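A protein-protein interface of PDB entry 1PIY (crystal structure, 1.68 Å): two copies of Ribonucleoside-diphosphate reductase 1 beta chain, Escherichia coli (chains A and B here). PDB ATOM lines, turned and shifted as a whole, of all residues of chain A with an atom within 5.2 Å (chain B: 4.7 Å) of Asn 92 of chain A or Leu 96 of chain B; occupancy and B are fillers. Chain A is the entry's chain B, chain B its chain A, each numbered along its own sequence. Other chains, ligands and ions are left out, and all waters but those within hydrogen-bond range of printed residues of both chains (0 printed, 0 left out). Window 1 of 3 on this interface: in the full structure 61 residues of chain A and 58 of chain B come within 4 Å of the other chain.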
ATOM      1  N   GLY A  88     -11.227   7.386  16.515  1.00  0.00           N
ATOM      2  CA  GLY A  88     -11.313   8.199  15.320  1.00  0.00           C
ATOM      3  C   GLY A  88      -9.934   8.460  14.741  1.00  0.00           C
ATOM      4  O   GLY A  88      -9.765   8.532  13.526  1.00  0.00           O
ATOM      5  N   ARG A  89      -8.931   8.561  15.609  1.00  0.00           N
ATOM      6  CA  ARG A  89      -7.577   8.859  15.159  1.00  0.00           C
ATOM      7  C   ARG A  89      -6.577   7.712  15.176  1.00  0.00           C
ATOM      8  O   ARG A  89      -5.738   7.601  14.287  1.00  0.00           O
ATOM      9  CB  ARG A  89      -6.991  10.008  16.004  1.00  0.00           C
ATOM     10  CG  ARG A  89      -6.600   9.614  17.446  1.00  0.00           C
ATOM     11  CD  ARG A  89      -6.046  10.815  18.228  1.00  0.00           C
ATOM     12  NE  ARG A  89      -7.051  11.863  18.362  1.00  0.00           N
ATOM     13  CZ  ARG A  89      -7.832  12.034  19.421  1.00  0.00           C
ATOM     14  NH1 ARG A  89      -7.728  11.230  20.474  1.00  0.00           N
ATOM     15  NH2 ARG A  89      -8.749  12.985  19.412  1.00  0.00           N
ATOM     16  N   SER A  90      -6.671   6.858  16.185  1.00  0.00           N
ATOM     17  CA  SER A  90      -5.696   5.794  16.363  1.00  0.00           C
ATOM     18  C   SER A  90      -5.517   4.743  15.279  1.00  0.00           C
ATOM     19  O   SER A  90      -4.383   4.384  14.955  1.00  0.00           O
ATOM     20  CB  SER A  90      -5.923   5.147  17.728  1.00  0.00           C
ATOM     21  OG  SER A  90      -5.957   6.162  18.721  1.00  0.00           O
ATOM     22  N   PRO A  91      -6.615   4.216  14.710  1.00  0.00           N
ATOM     23  CA  PRO A  91      -6.385   3.216  13.664  1.00  0.00           C
ATOM     24  C   PRO A  91      -5.550   3.839  12.541  1.00  0.00           C
ATOM     25  O   PRO A  91      -4.666   3.193  11.970  1.00  0.00           O
ATOM     26  CB  PRO A  91      -7.804   2.854  13.223  1.00  0.00           C
ATOM     27  CG  PRO A  91      -8.568   2.954  14.507  1.00  0.00           C
ATOM     28  CD  PRO A  91      -8.035   4.257  15.097  1.00  0.00           C
ATOM     29  N   ASN A  92      -5.814   5.106  12.243  1.00  0.00           N
ATOM     30  CA  ASN A  92      -5.068   5.788  11.195  1.00  0.00           C
ATOM     31  C   ASN A  92      -3.603   5.996  11.553  1.00  0.00           C
ATOM     32  O   ASN A  92      -2.718   5.585  10.809  1.00  0.00           O
ATOM     33  CB  ASN A  92      -5.695   7.143  10.850  1.00  0.00           C
ATOM     34  CG  ASN A  92      -6.899   7.014   9.929  1.00  0.00           C
ATOM     35  OD1 ASN A  92      -7.005   6.060   9.160  1.00  0.00           O
ATOM     36  ND2 ASN A  92      -7.795   7.984   9.988  1.00  0.00           N
ATOM     37  N   VAL A  93      -3.343   6.614  12.698  1.00  0.00           N
ATOM     38  CA  VAL A  93      -1.966   6.888  13.096  1.00  0.00           C
ATOM     39  C   VAL A  93      -1.136   5.650  13.396  1.00  0.00           C
ATOM     40  O   VAL A  93       0.064   5.616  13.098  1.00  0.00           O
ATOM     41  CB  VAL A  93      -1.924   7.820  14.322  1.00  0.00           C
ATOM     42  CG1 VAL A  93      -0.473   8.098  14.725  1.00  0.00           C
ATOM     43  CG2 VAL A  93      -2.634   9.126  13.982  1.00  0.00           C
ATOM     44  N   ALA A  94      -1.774   4.629  13.961  1.00  0.00           N
ATOM     45  CA  ALA A  94      -1.078   3.398  14.323  1.00  0.00           C
ATOM     46  C   ALA A  94      -0.949   2.343  13.224  1.00  0.00           C
ATOM     47  O   ALA A  94       0.095   1.696  13.097  1.00  0.00           O
ATOM     48  CB  ALA A  94      -1.755   2.778  15.542  1.00  0.00           C
ATOM     49  N   LEU A  95      -1.995   2.173  12.424  1.00  0.00           N
ATOM     50  CA  LEU A  95      -1.973   1.138  11.395  1.00  0.00           C
ATOM     51  C   LEU A  95      -1.542   1.521   9.985  1.00  0.00           C
ATOM     52  O   LEU A  95      -0.848   0.751   9.320  1.00  0.00           O
ATOM     53  CB  LEU A  95      -3.342   0.458  11.348  1.00  0.00           C
ATOM     54  CG  LEU A  95      -3.820  -0.059  12.705  1.00  0.00           C
ATOM     55  CD1 LEU A  95      -5.194  -0.699  12.559  1.00  0.00           C
ATOM     56  CD2 LEU A  95      -2.810  -1.080  13.257  1.00  0.00           C
ATOM     57  N   LEU A  96      -1.944   2.696   9.516  1.00  0.00           N
ATOM     58  CA  LEU A  96      -1.579   3.118   8.165  1.00  0.00           C
ATOM     59  C   LEU A  96      -0.096   2.988   7.825  1.00  0.00           C
ATOM     60  O   LEU A  96       0.267   2.563   6.723  1.00  0.00           O
ATOM     61  CB  LEU A  96      -2.022   4.566   7.916  1.00  0.00           C
ATOM     62  CG  LEU A  96      -3.495   4.802   7.598  1.00  0.00           C
ATOM     63  CD1 LEU A  96      -4.360   4.181   8.663  1.00  0.00           C
ATOM     64  CD2 LEU A  96      -3.764   6.288   7.493  1.00  0.00           C
ATOM     65  N   PRO A  97       0.790   3.353   8.762  1.00  0.00           N
ATOM     66  CA  PRO A  97       2.219   3.247   8.466  1.00  0.00           C
ATOM     67  C   PRO A  97       2.717   1.808   8.388  1.00  0.00           C
ATOM     68  O   PRO A  97       3.881   1.568   8.072  1.00  0.00           O
ATOM     69  CB  PRO A  97       2.871   4.013   9.623  1.00  0.00           C
ATOM     70  CG  PRO A  97       1.790   4.977  10.056  1.00  0.00           C
ATOM     71  CD  PRO A  97       0.569   4.103  10.011  1.00  0.00           C
ATOM     72  N   VAL A 108      -9.206   0.553   6.985  1.00  0.00           N
ATOM     73  CA  VAL A 108      -8.830   1.250   8.204  1.00  0.00           C
ATOM     74  C   VAL A 108      -9.236   2.718   8.165  1.00  0.00           C
ATOM     75  O   VAL A 108      -9.738   3.250   9.154  1.00  0.00           O
ATOM     76  CB  VAL A 108      -7.319   1.118   8.476  1.00  0.00           C
ATOM     77  CG1 VAL A 108      -6.904   2.062   9.576  1.00  0.00           C
ATOM     78  CG2 VAL A 108      -7.004  -0.312   8.876  1.00  0.00           C
ATOM     79  N   GLU A 109      -9.041   3.372   7.026  1.00  0.00           N
ATOM     80  CA  GLU A 109      -9.411   4.780   6.914  1.00  0.00           C
ATOM     81  C   GLU A 109     -10.923   4.957   6.946  1.00  0.00           C
ATOM     82  O   GLU A 109     -11.426   5.950   7.458  1.00  0.00           O
ATOM     83  CB  GLU A 109      -8.831   5.387   5.635  1.00  0.00           C
ATOM     84  CG  GLU A 109      -7.319   5.241   5.562  1.00  0.00           C
ATOM     85  CD  GLU A 109      -6.678   6.164   4.561  1.00  0.00           C
ATOM     86  OE1 GLU A 109      -6.562   7.378   4.857  1.00  0.00           O
ATOM     87  OE2 GLU A 109      -6.288   5.677   3.483  1.00  0.00           O
ATOM     88  N   ALA A 112     -11.954   4.281  10.662  1.00  0.00           N
ATOM     89  CA  ALA A 112     -11.622   5.447  11.480  1.00  0.00           C
ATOM     90  C   ALA A 112     -12.602   6.580  11.200  1.00  0.00           C
ATOM     91  O   ALA A 112     -13.098   7.233  12.122  1.00  0.00           O
ATOM     92  CB  ALA A 112     -10.195   5.896  11.194  1.00  0.00           C
ATOM     93  N   TYR B   2       4.406  11.004  21.002  1.00  0.00           N
ATOM     94  CA  TYR B   2       3.051  11.199  20.513  1.00  0.00           C
ATOM     95  C   TYR B   2       2.115  10.333  21.346  1.00  0.00           C
ATOM     96  O   TYR B   2       2.486   9.235  21.766  1.00  0.00           O
ATOM     97  CB  TYR B   2       2.933  10.770  19.047  1.00  0.00           C
ATOM     98  CG  TYR B   2       1.507  10.789  18.542  1.00  0.00           C
ATOM     99  CD1 TYR B   2       0.880  11.994  18.225  1.00  0.00           C
ATOM    100  CD2 TYR B   2       0.764   9.612  18.437  1.00  0.00           C
ATOM    101  CE1 TYR B   2      -0.446  12.033  17.821  1.00  0.00           C
ATOM    102  CE2 TYR B   2      -0.572   9.640  18.034  1.00  0.00           C
ATOM    103  CZ  TYR B   2      -1.169  10.854  17.727  1.00  0.00           C
ATOM    104  OH  TYR B   2      -2.490  10.908  17.333  1.00  0.00           O
ATOM    105  N   PRO B  91      -2.563  12.806   4.084  1.00  0.00           N
ATOM    106  CA  PRO B  91      -3.004  13.769   5.100  1.00  0.00           C
ATOM    107  C   PRO B  91      -3.054  13.103   6.481  1.00  0.00           C
ATOM    108  O   PRO B  91      -2.664  13.700   7.491  1.00  0.00           O
ATOM    109  CB  PRO B  91      -4.384  14.181   4.597  1.00  0.00           C
ATOM    110  CG  PRO B  91      -4.196  14.145   3.104  1.00  0.00           C
ATOM    111  CD  PRO B  91      -3.451  12.840   2.906  1.00  0.00           C
ATOM    112  N   ASN B  92      -3.525  11.859   6.523  1.00  0.00           N
ATOM    113  CA  ASN B  92      -3.611  11.135   7.789  1.00  0.00           C
ATOM    114  C   ASN B  92      -2.246  10.787   8.371  1.00  0.00           C
ATOM    115  O   ASN B  92      -2.002  10.992   9.556  1.00  0.00           O
ATOM    116  CB  ASN B  92      -4.417   9.841   7.629  1.00  0.00           C
ATOM    117  CG  ASN B  92      -5.909  10.085   7.574  1.00  0.00           C
ATOM    118  OD1 ASN B  92      -6.419  10.991   8.226  1.00  0.00           O
ATOM    119  ND2 ASN B  92      -6.623   9.260   6.809  1.00  0.00           N
ATOM    120  N   ALA B  94       0.829  12.101   7.559  1.00  0.00           N
ATOM    121  CA  ALA B  94       1.718  13.238   7.756  1.00  0.00           C
ATOM    122  C   ALA B  94       1.193  14.370   8.629  1.00  0.00           C
ATOM    123  O   ALA B  94       1.944  14.954   9.407  1.00  0.00           O
ATOM    124  CB  ALA B  94       2.144  13.793   6.389  1.00  0.00           C
ATOM    125  N   LEU B  95      -0.095  14.674   8.522  1.00  0.00           N
ATOM    126  CA  LEU B  95      -0.655  15.780   9.288  1.00  0.00           C
ATOM    127  C   LEU B  95      -1.312  15.398  10.600  1.00  0.00           C
ATOM    128  O   LEU B  95      -1.159  16.091  11.605  1.00  0.00           O
ATOM    129  CB  LEU B  95      -1.657  16.550   8.413  1.00  0.00           C
ATOM    130  CG  LEU B  95      -1.144  16.931   7.019  1.00  0.00           C
ATOM    131  CD1 LEU B  95      -2.241  17.652   6.238  1.00  0.00           C
ATOM    132  CD2 LEU B  95       0.087  17.821   7.144  1.00  0.00           C
ATOM    133  N   LEU B  96      -2.040  14.290  10.601  1.00  0.00           N
ATOM    134  CA  LEU B  96      -2.751  13.854  11.790  1.00  0.00           C
ATOM    135  C   LEU B  96      -1.909  13.855  13.075  1.00  0.00           C
ATOM    136  O   LEU B  96      -2.369  14.308  14.127  1.00  0.00           O
ATOM    137  CB  LEU B  96      -3.361  12.473  11.525  1.00  0.00           C
ATOM    138  CG  LEU B  96      -4.514  11.987  12.388  1.00  0.00           C
ATOM    139  CD1 LEU B  96      -5.539  13.095  12.587  1.00  0.00           C
ATOM    140  CD2 LEU B  96      -5.142  10.770  11.704  1.00  0.00           C
ATOM    141  N   PRO B  97      -0.661  13.366  13.011  1.00  0.00           N
ATOM    142  CA  PRO B  97       0.169  13.350  14.219  1.00  0.00           C
ATOM    143  C   PRO B  97       0.603  14.729  14.712  1.00  0.00           C
ATOM    144  O   PRO B  97       1.141  14.845  15.812  1.00  0.00           O
ATOM    145  CB  PRO B  97       1.375  12.504  13.806  1.00  0.00           C
ATOM    146  CG  PRO B  97       0.825  11.619  12.722  1.00  0.00           C
ATOM    147  CD  PRO B  97      -0.029  12.581  11.937  1.00  0.00           C
ATOM    148  N   LEU B  98       0.362  15.770  13.915  1.00  0.00           N
ATOM    149  CA  LEU B  98       0.781  17.125  14.286  1.00  0.00           C
ATOM    150  C   LEU B  98      -0.323  18.118  14.623  1.00  0.00           C
ATOM    151  O   LEU B  98      -0.035  19.265  14.978  1.00  0.00           O
ATOM    152  CB  LEU B  98       1.619  17.730  13.160  1.00  0.00           C
ATOM    153  CG  LEU B  98       2.839  16.931  12.712  1.00  0.00           C
ATOM    154  CD1 LEU B  98       3.504  17.624  11.525  1.00  0.00           C
ATOM    155  CD2 LEU B  98       3.803  16.806  13.884  1.00  0.00           C
ATOM    156  N   ILE B  99      -1.578  17.695  14.515  1.00  0.00           N
ATOM    157  CA  ILE B  99      -2.700  18.587  14.774  1.00  0.00           C
ATOM    158  C   ILE B  99      -3.075  18.689  16.246  1.00  0.00           C
ATOM    159  O   ILE B  99      -3.128  17.684  16.954  1.00  0.00           O
ATOM    160  CB  ILE B  99      -3.926  18.145  13.953  1.00  0.00           C
ATOM    161  CG1 ILE B  99      -3.592  18.265  12.467  1.00  0.00           C
ATOM    162  CG2 ILE B  99      -5.149  18.997  14.300  1.00  0.00           C
ATOM    163  CD1 ILE B  99      -4.569  17.550  11.564  1.00  0.00           C
ATOM    164  N   GLU B 105      -8.421  18.261  13.168  1.00  0.00           N
ATOM    165  CA  GLU B 105      -8.122  16.831  13.150  1.00  0.00           C
ATOM    166  C   GLU B 105      -9.196  16.086  12.360  1.00  0.00           C
ATOM    167  O   GLU B 105      -8.898  15.277  11.481  1.00  0.00           O
ATOM    168  CB  GLU B 105      -8.074  16.270  14.570  1.00  0.00           C
ATOM    169  CG  GLU B 105      -7.733  14.783  14.603  1.00  0.00           C
ATOM    170  CD  GLU B 105      -7.851  14.186  15.987  1.00  0.00           C
ATOM    171  OE1 GLU B 105      -8.987  14.083  16.499  1.00  0.00           O
ATOM    172  OE2 GLU B 105      -6.803  13.820  16.554  1.00  0.00           O
ATOM    173  N   GLU B 109      -9.147  14.096   8.560  1.00  0.00           N
ATOM    174  CA  GLU B 109      -9.574  12.715   8.403  1.00  0.00           C
ATOM    175  C   GLU B 109     -10.745  12.600   7.428  1.00  0.00           C
ATOM    176  O   GLU B 109     -10.847  11.626   6.678  1.00  0.00           O
ATOM    177  CB  GLU B 109      -9.943  12.124   9.764  1.00  0.00           C
ATOM    178  CG  GLU B 109      -8.740  11.981  10.681  1.00  0.00           C
ATOM    179  CD  GLU B 109      -9.030  11.150  11.914  1.00  0.00           C
ATOM    180  OE1 GLU B 109      -9.492  11.716  12.924  1.00  0.00           O
ATOM    181  OE2 GLU B 109      -8.797   9.923  11.867  1.00  0.00           O
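O of Pro 91 of chain B lies within hydrogen-bond range of N of Leu 96 of chain B.
Among the printed residues, merely in contact across the chains: Arg 89 of chain A with Tyr 2 of chain B (3.7 Å), Arg 89 of chain A with Glu 109 of chain B (3.7 Å), Asn 92 of chain A with Asn 92 of chain B (3.6 Å), Asn 92 of chain A with Leu 96 of chain B (3.8 Å), Val 93 of chain A with Tyr 2 of chain B (3.7 Å), Val 93 of chain A with Leu 96 of chain B (3.8 Å) and Leu 96 of chain A with Asn 92 of chain B (3.6 Å).
Hydrophobic or aromatic side chains of chain B that line the printed part of chain A: Tyr 2 and Leu 96.
Printed residues of chain A that touch a printed residue of chain B: Gly 88, Arg 89, Asn 92, Val 93, Leu 96 and Glu 109.
Hydrophobic or aromatic side chains of chain A within 4 Å of the printed part of chain B: Val 93 and Leu 96.
Among the printed residues, Asp or Glu carboxylates within 4 Å of a Lys or Arg side-chain nitrogen of the other chain: Arg 89 of chain A with Glu 105 of chain B (2.7 Å).
The side-chain carboxylate of Glu 105 of chain B lies within salt-bridge range of the guanidinium group of Arg 89 of chain A (2.7 Å).
The side-chain carboxylate (OE2) of Glu 109 of chain B is in hydrogen-bond range of the side-chain amide nitrogen (ND2) of Asn 92 of chain A.
The side-chain carboxylate of Glu 109 of chain A is in hydrogen-bond range of the side-chain amide nitrogen of Asn 92 of chain B, at 2.7 Å.
The backbone carbonyl oxygen of Gly 88 of chain A lies close to the side-chain carboxylate of Glu 109 of chain B (2.4 Å).
Asn 92 of chain A touches its own counterpart, Asn 92 of chain B.
Asn 92 of chain A touches Leu 96 of chain B, and with the chains exchanged Leu 96 of chain A touches Asn 92 of chain B.
Asn 92 of chain A touches Glu 109 of chain B, and with the chains exchanged Glu 109 of chain A touches Asn 92 of chain B.
Of the printed residues of chain B, Gly 88 of chain A touches Glu 109.
Asn 92 of chain A touches just these residues of chain B: Asn 92 (3.6 Å), Leu 96 (3.8 Å) and Glu 109 (2.9 Å).
Of the printed residues of chain B, Leu 96 of chain A touches Asn 92 (3.6 Å).
Pro 97 of chain A touches none of the printed residues of chain B.
Val 108 of chain A touches none of the printed residues of chain B.
Of the printed residues of chain B, Glu 109 of chain A touches Asn 92.
Of chain A, only Asn 92 (3.8 Å) and Val 93 (3.8 Å) come within 4 Å of Leu 96 of chain B.
The nearest residue of chain A that does not touch Leu 96 of chain B is Arg 89 of chain A (4.1 Å).
The nearest printed residue of chain B that does not touch Leu 96 of chain A is Leu 96 of chain B (6.3 Å).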
